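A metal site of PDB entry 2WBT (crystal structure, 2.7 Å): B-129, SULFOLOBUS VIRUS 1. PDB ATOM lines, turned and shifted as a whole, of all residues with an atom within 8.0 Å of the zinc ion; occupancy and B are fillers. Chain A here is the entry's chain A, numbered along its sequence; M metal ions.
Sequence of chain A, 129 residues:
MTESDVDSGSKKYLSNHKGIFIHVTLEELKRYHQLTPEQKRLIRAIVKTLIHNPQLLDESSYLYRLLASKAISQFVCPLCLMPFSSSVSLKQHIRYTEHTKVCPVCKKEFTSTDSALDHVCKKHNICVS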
ATOM      1  N   VAL A  76     -20.474   7.442 -14.629  1.00  0.00           N
ATOM      2  CA  VAL A  76     -20.465   6.362 -15.615  1.00  0.00           C
ATOM      3  C   VAL A  76     -19.311   5.404 -15.341  1.00  0.00           C
ATOM      4  O   VAL A  76     -18.247   5.809 -14.864  1.00  0.00           O
ATOM      5  CB  VAL A  76     -20.316   6.915 -17.047  1.00  0.00           C
ATOM      6  CG1 VAL A  76     -20.482   5.802 -18.073  1.00  0.00           C
ATOM      7  CG2 VAL A  76     -21.333   8.024 -17.301  1.00  0.00           C
ATOM      8  N   CYS A  77     -19.541   4.140 -15.633  1.00  0.00           N
ATOM      9  CA  CYS A  77     -18.526   3.096 -15.476  1.00  0.00           C
ATOM     10  C   CYS A  77     -17.725   2.953 -16.772  1.00  0.00           C
ATOM     11  O   CYS A  77     -18.303   2.744 -17.846  1.00  0.00           O
ATOM     12  CB  CYS A  77     -19.186   1.763 -15.120  1.00  0.00           C
ATOM     13  SG  CYS A  77     -18.033   0.431 -14.790  1.00  0.00           S
ATOM     14  N   PRO A  78     -16.388   3.038 -16.690  1.00  0.00           N
ATOM     15  CA  PRO A  78     -15.564   2.947 -17.899  1.00  0.00           C
ATOM     16  C   PRO A  78     -15.667   1.591 -18.605  1.00  0.00           C
ATOM     17  O   PRO A  78     -15.587   1.539 -19.837  1.00  0.00           O
ATOM     18  CB  PRO A  78     -14.140   3.180 -17.389  1.00  0.00           C
ATOM     19  CG  PRO A  78     -14.311   3.815 -16.049  1.00  0.00           C
ATOM     20  CD  PRO A  78     -15.551   3.209 -15.492  1.00  0.00           C
ATOM     21  N   LEU A  79     -15.827   0.525 -17.832  1.00  0.00           N
ATOM     22  CA  LEU A  79     -15.864  -0.833 -18.392  1.00  0.00           C
ATOM     23  C   LEU A  79     -17.185  -1.168 -19.092  1.00  0.00           C
ATOM     24  O   LEU A  79     -17.177  -1.785 -20.154  1.00  0.00           O
ATOM     25  CB  LEU A  79     -15.552  -1.870 -17.319  1.00  0.00           C
ATOM     26  CG  LEU A  79     -14.228  -1.693 -16.557  1.00  0.00           C
ATOM     27  CD1 LEU A  79     -14.058  -2.822 -15.546  1.00  0.00           C
ATOM     28  CD2 LEU A  79     -13.045  -1.635 -17.508  1.00  0.00           C
ATOM     29  N   CYS A  80     -18.320  -0.763 -18.514  1.00  0.00           N
ATOM     30  CA  CYS A  80     -19.620  -1.027 -19.168  1.00  0.00           C
ATOM     31  C   CYS A  80     -20.317   0.204 -19.760  1.00  0.00           C
ATOM     32  O   CYS A  80     -21.254   0.059 -20.555  1.00  0.00           O
ATOM     33  CB  CYS A  80     -20.568  -1.791 -18.252  1.00  0.00           C
ATOM     34  SG  CYS A  80     -21.184  -0.822 -16.772  1.00  0.00           S
ATOM     35  N   LEU A  81     -19.845   1.407 -19.432  1.00  0.00           N
ATOM     36  CA  LEU A  81     -20.416   2.649 -19.987  1.00  0.00           C
ATOM     37  C   LEU A  81     -21.884   2.875 -19.612  1.00  0.00           C
ATOM     38  O   LEU A  81     -22.629   3.471 -20.387  1.00  0.00           O
ATOM     39  CB  LEU A  81     -20.280   2.688 -21.519  1.00  0.00           C
ATOM     40  CG  LEU A  81     -18.847   2.752 -22.053  1.00  0.00           C
ATOM     41  CD1 LEU A  81     -18.859   2.625 -23.571  1.00  0.00           C
ATOM     42  CD2 LEU A  81     -18.157   4.035 -21.627  1.00  0.00           C
ATOM     43  N   MET A  82     -22.290   2.369 -18.445  1.00  0.00           N
ATOM     44  CA  MET A  82     -23.661   2.535 -17.958  1.00  0.00           C
ATOM     45  C   MET A  82     -23.731   3.632 -16.884  1.00  0.00           C
ATOM     46  O   MET A  82     -22.931   3.620 -15.938  1.00  0.00           O
ATOM     47  CB  MET A  82     -24.220   1.218 -17.405  1.00  0.00           C
ATOM     48  CG  MET A  82     -24.369   0.091 -18.437  1.00  0.00           C
ATOM     49  SD  MET A  82     -25.434   0.452 -19.860  1.00  0.00           S
ATOM     50  CE  MET A  82     -24.236   0.977 -21.076  1.00  0.00           C
ATOM     51  N   PHE A  84     -25.056   5.889 -13.686  1.00  0.00           N
ATOM     52  CA  PHE A  84     -25.627   5.626 -12.370  1.00  0.00           C
ATOM     53  C   PHE A  84     -26.091   6.916 -11.713  1.00  0.00           C
ATOM     54  O   PHE A  84     -25.617   7.999 -12.050  1.00  0.00           O
ATOM     55  CB  PHE A  84     -24.609   4.898 -11.497  1.00  0.00           C
ATOM     56  CG  PHE A  84     -24.427   3.464 -11.874  1.00  0.00           C
ATOM     57  CD1 PHE A  84     -25.218   2.474 -11.307  1.00  0.00           C
ATOM     58  CD2 PHE A  84     -23.484   3.096 -12.827  1.00  0.00           C
ATOM     59  CE1 PHE A  84     -25.073   1.150 -11.670  1.00  0.00           C
ATOM     60  CE2 PHE A  84     -23.330   1.770 -13.194  1.00  0.00           C
ATOM     61  CZ  PHE A  84     -24.120   0.802 -12.606  1.00  0.00           C
ATOM     62  N   LEU A  90     -22.495   4.159  -8.206  1.00  0.00           N
ATOM     63  CA  LEU A  90     -21.506   3.839  -9.231  1.00  0.00           C
ATOM     64  C   LEU A  90     -20.404   2.919  -8.690  1.00  0.00           C
ATOM     65  O   LEU A  90     -20.026   1.959  -9.348  1.00  0.00           O
ATOM     66  CB  LEU A  90     -20.876   5.111  -9.801  1.00  0.00           C
ATOM     67  CG  LEU A  90     -19.641   4.940 -10.697  1.00  0.00           C
ATOM     68  CD1 LEU A  90     -20.002   4.220 -11.981  1.00  0.00           C
ATOM     69  CD2 LEU A  90     -19.011   6.293 -10.999  1.00  0.00           C
ATOM     70  N   HIS A  93     -21.474  -0.553  -7.782  1.00  0.00           N
ATOM     71  CA  HIS A  93     -21.458  -1.356  -9.008  1.00  0.00           C
ATOM     72  C   HIS A  93     -20.055  -1.852  -9.324  1.00  0.00           C
ATOM     73  O   HIS A  93     -19.855  -3.021  -9.655  1.00  0.00           O
ATOM     74  CB  HIS A  93     -21.995  -0.563 -10.197  1.00  0.00           C
ATOM     75  CG  HIS A  93     -21.615  -1.124 -11.543  1.00  0.00           C
ATOM     76  ND1 HIS A  93     -22.288  -2.167 -12.137  1.00  0.00           N
ATOM     77  CD2 HIS A  93     -20.654  -0.746 -12.420  1.00  0.00           C
ATOM     78  CE1 HIS A  93     -21.740  -2.421 -13.324  1.00  0.00           C
ATOM     79  NE2 HIS A  93     -20.755  -1.570 -13.515  1.00  0.00           N
ATOM     80  N   ILE A  94     -19.087  -0.939  -9.252  1.00  0.00           N
ATOM     81  CA  ILE A  94     -17.691  -1.279  -9.555  1.00  0.00           C
ATOM     82  C   ILE A  94     -17.145  -2.281  -8.541  1.00  0.00           C
ATOM     83  O   ILE A  94     -16.457  -3.233  -8.912  1.00  0.00           O
ATOM     84  CB  ILE A  94     -16.804  -0.024  -9.592  1.00  0.00           C
ATOM     85  CG1 ILE A  94     -17.019   0.734 -10.916  1.00  0.00           C
ATOM     86  CG2 ILE A  94     -15.324  -0.389  -9.466  1.00  0.00           C
ATOM     87  CD1 ILE A  94     -16.330   2.073 -10.972  1.00  0.00           C
ATOM     88  N   THR A  97     -20.404  -5.458  -8.652  1.00  0.00           N
ATOM     89  CA  THR A  97     -21.169  -5.896  -9.835  1.00  0.00           C
ATOM     90  C   THR A  97     -20.403  -5.924 -11.171  1.00  0.00           C
ATOM     91  O   THR A  97     -20.805  -6.641 -12.086  1.00  0.00           O
ATOM     92  CB  THR A  97     -22.440  -5.021 -10.000  1.00  0.00           C
ATOM     93  OG1 THR A  97     -23.125  -4.921  -8.748  1.00  0.00           O
ATOM     94  CG2 THR A  97     -23.383  -5.621 -11.048  1.00  0.00           C
ATOM     95  N   GLU A  98     -19.307  -5.169 -11.276  1.00  0.00           N
ATOM     96  CA  GLU A  98     -18.555  -5.097 -12.533  1.00  0.00           C
ATOM     97  C   GLU A  98     -17.490  -6.197 -12.609  1.00  0.00           C
ATOM     98  O   GLU A  98     -16.514  -6.173 -11.850  1.00  0.00           O
ATOM     99  CB  GLU A  98     -17.904  -3.716 -12.682  1.00  0.00           C
ATOM    100  CG  GLU A  98     -17.091  -3.514 -13.962  1.00  0.00           C
ATOM    101  CD  GLU A  98     -17.816  -4.015 -15.203  1.00  0.00           C
ATOM    102  OE1 GLU A  98     -18.820  -3.376 -15.599  1.00  0.00           O
ATOM    103  OE2 GLU A  98     -17.389  -5.036 -15.762  1.00  0.00           O
ATOM    104  N   HIS A  99     -17.687  -7.154 -13.516  1.00  0.00           N
ATOM    105  CA  HIS A  99     -16.821  -8.342 -13.612  1.00  0.00           C
ATOM    106  C   HIS A  99     -16.053  -8.502 -14.928  1.00  0.00           C
ATOM    107  O   HIS A  99     -15.418  -9.536 -15.138  1.00  0.00           O
ATOM    108  CB  HIS A  99     -17.645  -9.615 -13.375  1.00  0.00           C
ATOM    109  CG  HIS A  99     -18.341  -9.641 -12.054  1.00  0.00           C
ATOM    110  ND1 HIS A  99     -17.664  -9.573 -10.847  1.00  0.00           N
ATOM    111  CD2 HIS A  99     -19.658  -9.741 -11.737  1.00  0.00           C
ATOM    112  CE1 HIS A  99     -18.535  -9.622  -9.856  1.00  0.00           C
ATOM    113  NE2 HIS A  99     -19.748  -9.719 -10.372  1.00  0.00           N
ATOM    114  N   THR A 100     -16.094  -7.510 -15.815  1.00  0.00           N
ATOM    115  CA  THR A 100     -15.407  -7.623 -17.111  1.00  0.00           C
ATOM    116  C   THR A 100     -13.881  -7.566 -16.951  1.00  0.00           C
ATOM    117  O   THR A 100     -13.359  -6.730 -16.212  1.00  0.00           O
ATOM    118  CB  THR A 100     -15.845  -6.538 -18.114  1.00  0.00           C
ATOM    119  OG1 THR A 100     -15.308  -6.848 -19.414  1.00  0.00           O
ATOM    120  CG2 THR A 100     -15.347  -5.180 -17.688  1.00  0.00           C
ATOM    121  N   LEU A 117      -9.551  -1.838 -14.828  1.00  0.00           N
ATOM    122  CA  LEU A 117      -9.830  -0.430 -14.489  1.00  0.00           C
ATOM    123  C   LEU A 117      -8.583   0.442 -14.578  1.00  0.00           C
ATOM    124  O   LEU A 117      -8.589   1.474 -15.254  1.00  0.00           O
ATOM    125  CB  LEU A 117     -10.414  -0.307 -13.073  1.00  0.00           C
ATOM    126  CG  LEU A 117     -11.918  -0.536 -12.887  1.00  0.00           C
ATOM    127  CD1 LEU A 117     -12.317  -0.230 -11.457  1.00  0.00           C
ATOM    128  CD2 LEU A 117     -12.750   0.284 -13.865  1.00  0.00           C
HETATM  129 ZN    ZN M   1     -19.451  -1.317 -15.415  1.00  0.00          ZN
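Of the 16 residues printed, 4 come within 4 Å of the zinc ion.
The zinc ion is bound by OE1 of Glu 98 (2.2 Å), SG of Cys 80 (2.3 Å), NE2 of His 93 (2.3 Å) and SG of Cys 77 (2.3 Å). The zinc ion has four donor atoms within binding distance.
OE2 of Glu 98 sits at hydrogen-bond distance from N of Thr 100. The backbone NH (N) of Met 82 lies close to the side-chain sulfur (SG) of Cys 80, 3.8 Å away. N of Leu 79 sits close to SG of Cys 77 (3.8 Å). The backbone NH of Cys 77 lies within hydrogen-bond range of the backbone carbonyl oxygen of Met 82, 3.4 Å away.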
